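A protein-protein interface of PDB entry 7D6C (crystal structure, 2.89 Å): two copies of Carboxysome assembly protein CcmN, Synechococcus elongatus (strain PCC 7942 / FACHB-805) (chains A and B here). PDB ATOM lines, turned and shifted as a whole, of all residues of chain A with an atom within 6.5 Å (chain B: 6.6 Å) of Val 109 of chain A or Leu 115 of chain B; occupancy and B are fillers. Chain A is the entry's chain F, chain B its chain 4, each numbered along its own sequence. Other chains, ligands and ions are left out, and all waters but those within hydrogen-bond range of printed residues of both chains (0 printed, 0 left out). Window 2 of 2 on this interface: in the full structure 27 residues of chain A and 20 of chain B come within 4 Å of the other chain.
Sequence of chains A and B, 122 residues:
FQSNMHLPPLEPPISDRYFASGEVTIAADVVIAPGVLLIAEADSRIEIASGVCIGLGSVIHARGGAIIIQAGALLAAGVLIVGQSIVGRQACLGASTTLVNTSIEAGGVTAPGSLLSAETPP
Among the printed residues, merely in contact across the chains: Pro 112 of chain A with Ser 96 of chain B (3.1 Å), Pro 112 of chain A with Gly 113 of chain B (3.3 Å), Ala 111 of chain A with Leu 115 of chain B (3.5 Å), Gly 94 of chain A with Thr 98 of chain B (3.6 Å), Pro 112 of chain A with Thr 98 of chain B (3.8 Å), Val 109 of chain A with Leu 115 of chain B (3.8 Å), Thr 110 of chain A with Leu 115 of chain B (3.8 Å) and Pro 112 of chain A with Ser 114 of chain B (3.9 Å).
Printed residues of chain B that touch a printed residue of chain A: Ser 96, Thr 98, Gly 113, Ser 114 and Leu 115. Hydrophobic or aromatic side chains of chain B within 4 Å of the printed part of chain A: Leu 115. Along chain B the printed residues that touch a printed residue of chain A span positions 96 to 115. Among the printed residues, no Asp or Glu carboxylate lies within 4 Å of a Lys or Arg side-chain nitrogen of the other chain.
2 positions are printed for both chains. Of the 8 pairs that touch across the chains among the printed residues, none has its exchanged pair printed and touching as well.
Val 109 of chain A touches just one residue of chain B: Leu 115 (3.8 Å). Printed residues of chain A within 4 Å of Ser 96 of chain B: Pro 112 (3.1 Å). Leu 99 of chain B touches none of the printed residues of chain A. Printed residues of chain A within 4 Å of Ser 114 of chain B: Pro 112. Leu 115 of chain B touches three residues of chain A. The nearest printed residue of chain B that does not touch Gly 94 of chain A is Ser 96 of chain B (5.6 Å).
The backbone NH (N) of Thr 98 of chain B is in hydrogen-bond range of the backbone carbonyl oxygen (O) of Ser 114 of chain B (2.9 Å). The backbone NH (N) of Leu 116 of chain B lies within hydrogen-bond range of the backbone carbonyl oxygen (O) of Thr 98 of chain B, at 2.9 Å. O of Ala 111 of chain B is in hydrogen-bond range of OG of Ser 114 of chain B, 2.9 Å away. The backbone NH of Thr 110 of chain A is in hydrogen-bond range of the backbone carbonyl oxygen of Cys 92 of chain A, at 2.8 Å. The backbone NH (N) of Gly 94 of chain A is in hydrogen-bond range of the backbone carbonyl oxygen (O) of Thr 110 of chain A, 2.8 Å away.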
ATOM      1  N   GLN A  90     -33.015  -6.499  -7.265  1.00  0.00           N
ATOM      2  CA  GLN A  90     -31.852  -7.207  -6.723  1.00  0.00           C
ATOM      3  C   GLN A  90     -30.879  -6.314  -5.941  1.00  0.00           C
ATOM      4  O   GLN A  90     -29.793  -6.774  -5.535  1.00  0.00           O
ATOM      5  CB  GLN A  90     -31.075  -7.940  -7.824  1.00  0.00           C
ATOM      6  CG  GLN A  90     -31.906  -8.936  -8.606  1.00  0.00           C
ATOM      7  CD  GLN A  90     -31.893 -10.327  -8.017  1.00  0.00           C
ATOM      8  OE1 GLN A  90     -32.415 -10.549  -6.924  1.00  0.00           O
ATOM      9  NE2 GLN A  90     -31.340 -11.285  -8.759  1.00  0.00           N
ATOM     10  N   ALA A  91     -31.239  -5.064  -5.679  1.00  0.00           N
ATOM     11  CA  ALA A  91     -30.351  -4.160  -4.960  1.00  0.00           C
ATOM     12  C   ALA A  91     -30.135  -4.609  -3.506  1.00  0.00           C
ATOM     13  O   ALA A  91     -30.905  -5.399  -2.950  1.00  0.00           O
ATOM     14  CB  ALA A  91     -30.914  -2.736  -5.001  1.00  0.00           C
ATOM     15  N   CYS A  92     -29.064  -4.076  -2.895  1.00  0.00           N
ATOM     16  CA  CYS A  92     -28.643  -4.395  -1.525  1.00  0.00           C
ATOM     17  C   CYS A  92     -28.255  -3.112  -0.808  1.00  0.00           C
ATOM     18  O   CYS A  92     -27.367  -2.392  -1.276  1.00  0.00           O
ATOM     19  CB  CYS A  92     -27.440  -5.325  -1.505  1.00  0.00           C
ATOM     20  SG  CYS A  92     -27.649  -6.804  -2.380  1.00  0.00           S
ATOM     21  N   LEU A  93     -28.866  -2.851   0.347  1.00  0.00           N
ATOM     22  CA  LEU A  93     -28.679  -1.593   1.063  1.00  0.00           C
ATOM     23  C   LEU A  93     -28.066  -1.882   2.427  1.00  0.00           C
ATOM     24  O   LEU A  93     -28.709  -2.509   3.278  1.00  0.00           O
ATOM     25  CB  LEU A  93     -30.004  -0.859   1.215  1.00  0.00           C
ATOM     26  CG  LEU A  93     -30.827  -0.567  -0.036  1.00  0.00           C
ATOM     27  CD1 LEU A  93     -31.885   0.468   0.327  1.00  0.00           C
ATOM     28  CD2 LEU A  93     -29.947  -0.072  -1.132  1.00  0.00           C
ATOM     29  N   GLY A  94     -26.832  -1.410   2.635  1.00  0.00           N
ATOM     30  CA  GLY A  94     -26.154  -1.648   3.892  1.00  0.00           C
ATOM     31  C   GLY A  94     -26.923  -1.091   5.073  1.00  0.00           C
ATOM     32  O   GLY A  94     -27.794  -0.238   4.935  1.00  0.00           O
ATOM     33  N   ILE A 104     -32.263   3.775  -6.559  1.00  0.00           N
ATOM     34  CA  ILE A 104     -31.122   2.882  -6.746  1.00  0.00           C
ATOM     35  C   ILE A 104     -31.324   2.042  -8.006  1.00  0.00           C
ATOM     36  O   ILE A 104     -32.357   1.373  -8.171  1.00  0.00           O
ATOM     37  CB  ILE A 104     -30.898   1.978  -5.521  1.00  0.00           C
ATOM     38  CG1 ILE A 104     -30.624   2.840  -4.289  1.00  0.00           C
ATOM     39  CG2 ILE A 104     -29.747   0.994  -5.765  1.00  0.00           C
ATOM     40  CD1 ILE A 104     -29.370   3.684  -4.426  1.00  0.00           C
ATOM     41  N   GLU A 105     -30.328   2.090  -8.887  1.00  0.00           N
ATOM     42  CA  GLU A 105     -30.218   1.180 -10.022  1.00  0.00           C
ATOM     43  C   GLU A 105     -30.377  -0.273  -9.575  1.00  0.00           C
ATOM     44  O   GLU A 105     -29.918  -0.669  -8.495  1.00  0.00           O
ATOM     45  CB  GLU A 105     -28.849   1.414 -10.693  1.00  0.00           C
ATOM     46  CG  GLU A 105     -27.619   1.284  -9.712  1.00  0.00           C
ATOM     47  CD  GLU A 105     -27.383   2.540  -8.812  1.00  0.00           C
ATOM     48  OE1 GLU A 105     -28.252   3.451  -8.780  1.00  0.00           O
ATOM     49  OE2 GLU A 105     -26.345   2.605  -8.102  1.00  0.00           O
ATOM     50  N   ALA A 106     -31.048  -1.069 -10.403  1.00  0.00           N
ATOM     51  CA  ALA A 106     -31.074  -2.507 -10.173  1.00  0.00           C
ATOM     52  C   ALA A 106     -29.670  -3.025  -9.873  1.00  0.00           C
ATOM     53  O   ALA A 106     -28.682  -2.545 -10.432  1.00  0.00           O
ATOM     54  CB  ALA A 106     -31.658  -3.226 -11.384  1.00  0.00           C
ATOM     55  N   GLY A 107     -29.582  -3.983  -8.953  1.00  0.00           N
ATOM     56  CA  GLY A 107     -28.320  -4.605  -8.612  1.00  0.00           C
ATOM     57  C   GLY A 107     -27.331  -3.709  -7.899  1.00  0.00           C
ATOM     58  O   GLY A 107     -26.256  -4.188  -7.513  1.00  0.00           O
ATOM     59  N   GLY A 108     -27.649  -2.428  -7.716  1.00  0.00           N
ATOM     60  CA  GLY A 108     -26.737  -1.543  -7.028  1.00  0.00           C
ATOM     61  C   GLY A 108     -26.648  -1.876  -5.554  1.00  0.00           C
ATOM     62  O   GLY A 108     -27.595  -2.362  -4.943  1.00  0.00           O
ATOM     63  N   VAL A 109     -25.484  -1.617  -4.972  1.00  0.00           N
ATOM     64  CA  VAL A 109     -25.212  -1.954  -3.578  1.00  0.00           C
ATOM     65  C   VAL A 109     -24.750  -0.709  -2.826  1.00  0.00           C
ATOM     66  O   VAL A 109     -23.905   0.045  -3.312  1.00  0.00           O
ATOM     67  CB  VAL A 109     -24.165  -3.079  -3.475  1.00  0.00           C
ATOM     68  CG1 VAL A 109     -23.924  -3.453  -2.012  1.00  0.00           C
ATOM     69  CG2 VAL A 109     -24.620  -4.282  -4.274  1.00  0.00           C
ATOM     70  N   THR A 110     -25.281  -0.515  -1.629  1.00  0.00           N
ATOM     71  CA  THR A 110     -25.012   0.664  -0.816  1.00  0.00           C
ATOM     72  C   THR A 110     -24.186   0.344   0.420  1.00  0.00           C
ATOM     73  O   THR A 110     -24.574  -0.512   1.222  1.00  0.00           O
ATOM     74  CB  THR A 110     -26.322   1.323  -0.395  1.00  0.00           C
ATOM     75  OG1 THR A 110     -26.939   1.952  -1.533  1.00  0.00           O
ATOM     76  CG2 THR A 110     -26.094   2.270   0.728  1.00  0.00           C
ATOM     77  N   ALA A 111     -23.089   1.084   0.601  1.00  0.00           N
ATOM     78  CA  ALA A 111     -22.237   0.880   1.768  1.00  0.00           C
ATOM     79  C   ALA A 111     -23.002   1.232   3.032  1.00  0.00           C
ATOM     80  O   ALA A 111     -23.763   2.204   3.045  1.00  0.00           O
ATOM     81  CB  ALA A 111     -20.972   1.731   1.700  1.00  0.00           C
ATOM     82  N   PRO A 112     -22.838   0.465   4.098  1.00  0.00           N
ATOM     83  CA  PRO A 112     -23.509   0.798   5.355  1.00  0.00           C
ATOM     84  C   PRO A 112     -23.204   2.229   5.771  1.00  0.00           C
ATOM     85  O   PRO A 112     -22.108   2.745   5.537  1.00  0.00           O
ATOM     86  CB  PRO A 112     -22.938  -0.229   6.338  1.00  0.00           C
ATOM     87  CG  PRO A 112     -21.756  -0.839   5.633  1.00  0.00           C
ATOM     88  CD  PRO A 112     -22.063  -0.777   4.195  1.00  0.00           C
ATOM     89  N   SER B  96     -22.524  -3.796  11.101  1.00  0.00           N
ATOM     90  CA  SER B  96     -22.997  -3.277   9.826  1.00  0.00           C
ATOM     91  C   SER B  96     -22.155  -3.764   8.653  1.00  0.00           C
ATOM     92  O   SER B  96     -22.210  -3.184   7.570  1.00  0.00           O
ATOM     93  CB  SER B  96     -23.037  -1.748   9.845  1.00  0.00           C
ATOM     94  OG  SER B  96     -24.078  -1.289  10.706  1.00  0.00           O
ATOM     95  N   THR B  97     -21.379  -4.826   8.841  1.00  0.00           N
ATOM     96  CA  THR B  97     -20.633  -5.399   7.733  1.00  0.00           C
ATOM     97  C   THR B  97     -21.616  -5.812   6.634  1.00  0.00           C
ATOM     98  O   THR B  97     -22.742  -6.244   6.910  1.00  0.00           O
ATOM     99  CB  THR B  97     -19.862  -6.634   8.186  1.00  0.00           C
ATOM    100  OG1 THR B  97     -19.139  -6.324   9.367  1.00  0.00           O
ATOM    101  CG2 THR B  97     -18.810  -6.926   7.176  1.00  0.00           C
ATOM    102  N   THR B  98     -21.195  -5.692   5.376  1.00  0.00           N
ATOM    103  CA  THR B  98     -22.059  -6.024   4.247  1.00  0.00           C
ATOM    104  C   THR B  98     -21.270  -6.849   3.238  1.00  0.00           C
ATOM    105  O   THR B  98     -20.364  -6.334   2.570  1.00  0.00           O
ATOM    106  CB  THR B  98     -22.626  -4.757   3.604  1.00  0.00           C
ATOM    107  OG1 THR B  98     -23.644  -4.205   4.453  1.00  0.00           O
ATOM    108  CG2 THR B  98     -23.223  -5.065   2.231  1.00  0.00           C
ATOM    109  N   LEU B  99     -21.631  -8.121   3.119  1.00  0.00           N
ATOM    110  CA  LEU B  99     -20.946  -9.085   2.272  1.00  0.00           C
ATOM    111  C   LEU B  99     -21.910  -9.502   1.179  1.00  0.00           C
ATOM    112  O   LEU B  99     -22.977 -10.049   1.476  1.00  0.00           O
ATOM    113  CB  LEU B  99     -20.518 -10.309   3.077  1.00  0.00           C
ATOM    114  CG  LEU B  99     -19.491 -10.084   4.183  1.00  0.00           C
ATOM    115  CD1 LEU B  99     -18.898 -11.410   4.629  1.00  0.00           C
ATOM    116  CD2 LEU B  99     -18.397  -9.142   3.720  1.00  0.00           C
ATOM    117  N   VAL B 100     -21.539  -9.241  -0.075  1.00  0.00           N
ATOM    118  CA  VAL B 100     -22.338  -9.618  -1.236  1.00  0.00           C
ATOM    119  C   VAL B 100     -21.455 -10.448  -2.147  1.00  0.00           C
ATOM    120  O   VAL B 100     -20.502  -9.924  -2.734  1.00  0.00           O
ATOM    121  CB  VAL B 100     -22.890  -8.404  -1.990  1.00  0.00           C
ATOM    122  CG1 VAL B 100     -23.943  -8.860  -2.996  1.00  0.00           C
ATOM    123  CG2 VAL B 100     -23.472  -7.395  -1.020  1.00  0.00           C
ATOM    124  N   THR B 102     -19.171 -12.569  -1.588  1.00  0.00           N
ATOM    125  CA  THR B 102     -17.776 -12.582  -1.161  1.00  0.00           C
ATOM    126  C   THR B 102     -17.666 -13.345   0.154  1.00  0.00           C
ATOM    127  O   THR B 102     -18.625 -13.410   0.931  1.00  0.00           O
ATOM    128  CB  THR B 102     -17.180 -11.160  -1.003  1.00  0.00           C
ATOM    129  OG1 THR B 102     -18.040 -10.364  -0.191  1.00  0.00           O
ATOM    130  CG2 THR B 102     -17.008 -10.458  -2.339  1.00  0.00           C
ATOM    131  N   ALA B 111     -13.677  -4.705   9.515  1.00  0.00           N
ATOM    132  CA  ALA B 111     -13.940  -3.501  10.280  1.00  0.00           C
ATOM    133  C   ALA B 111     -15.429  -3.172  10.219  1.00  0.00           C
ATOM    134  O   ALA B 111     -16.100  -3.482   9.232  1.00  0.00           O
ATOM    135  CB  ALA B 111     -13.140  -2.327   9.732  1.00  0.00           C
ATOM    136  N   PRO B 112     -15.972  -2.553  11.261  1.00  0.00           N
ATOM    137  CA  PRO B 112     -17.379  -2.143  11.213  1.00  0.00           C
ATOM    138  C   PRO B 112     -17.656  -1.261  10.008  1.00  0.00           C
ATOM    139  O   PRO B 112     -16.785  -0.536   9.518  1.00  0.00           O
ATOM    140  CB  PRO B 112     -17.585  -1.380  12.535  1.00  0.00           C
ATOM    141  CG  PRO B 112     -16.206  -1.245  13.170  1.00  0.00           C
ATOM    142  CD  PRO B 112     -15.387  -2.379  12.601  1.00  0.00           C
ATOM    143  N   GLY B 113     -18.889  -1.355   9.522  1.00  0.00           N
ATOM    144  CA  GLY B 113     -19.289  -0.631   8.338  1.00  0.00           C
ATOM    145  C   GLY B 113     -18.534  -1.002   7.092  1.00  0.00           C
ATOM    146  O   GLY B 113     -18.565  -0.243   6.123  1.00  0.00           O
ATOM    147  N   SER B 114     -17.858  -2.146   7.068  1.00  0.00           N
ATOM    148  CA  SER B 114     -17.125  -2.458   5.853  1.00  0.00           C
ATOM    149  C   SER B 114     -18.045  -3.139   4.849  1.00  0.00           C
ATOM    150  O   SER B 114     -19.083  -3.704   5.196  1.00  0.00           O
ATOM    151  CB  SER B 114     -15.885  -3.322   6.139  1.00  0.00           C
ATOM    152  OG  SER B 114     -16.209  -4.634   6.522  1.00  0.00           O
ATOM    153  N   LEU B 115     -17.664  -3.046   3.579  1.00  0.00           N
ATOM    154  CA  LEU B 115     -18.470  -3.558   2.476  1.00  0.00           C
ATOM    155  C   LEU B 115     -17.572  -4.330   1.527  1.00  0.00           C
ATOM    156  O   LEU B 115     -16.724  -3.742   0.846  1.00  0.00           O
ATOM    157  CB  LEU B 115     -19.179  -2.429   1.735  1.00  0.00           C
ATOM    158  CG  LEU B 115     -19.880  -2.797   0.428  1.00  0.00           C
ATOM    159  CD1 LEU B 115     -21.217  -2.104   0.312  1.00  0.00           C
ATOM    160  CD2 LEU B 115     -19.019  -2.405  -0.753  1.00  0.00           C
ATOM    161  N   LEU B 116     -17.768  -5.633   1.457  1.00  0.00           N
ATOM    162  CA  LEU B 116     -17.076  -6.460   0.486  1.00  0.00           C
ATOM    163  C   LEU B 116     -18.125  -6.972  -0.480  1.00  0.00           C
ATOM    164  O   LEU B 116     -19.174  -7.462  -0.053  1.00  0.00           O
ATOM    165  CB  LEU B 116     -16.322  -7.607   1.165  1.00  0.00           C
ATOM    166  CG  LEU B 116     -15.174  -7.172   2.092  1.00  0.00           C
ATOM    167  CD1 LEU B 116     -15.673  -6.672   3.450  1.00  0.00           C
ATOM    168  CD2 LEU B 116     -14.194  -8.303   2.311  1.00  0.00           C
ATOM    169  N   SER B 117     -17.855  -6.820  -1.772  1.00  0.00           N
ATOM    170  CA  SER B 117     -18.841  -7.111  -2.799  1.00  0.00           C
ATOM    171  C   SER B 117     -18.123  -7.468  -4.092  1.00  0.00           C
ATOM    172  O   SER B 117     -17.097  -6.868  -4.425  1.00  0.00           O
ATOM    173  CB  SER B 117     -19.775  -5.909  -3.008  1.00  0.00           C
ATOM    174  OG  SER B 117     -20.480  -5.967  -4.239  1.00  0.00           O
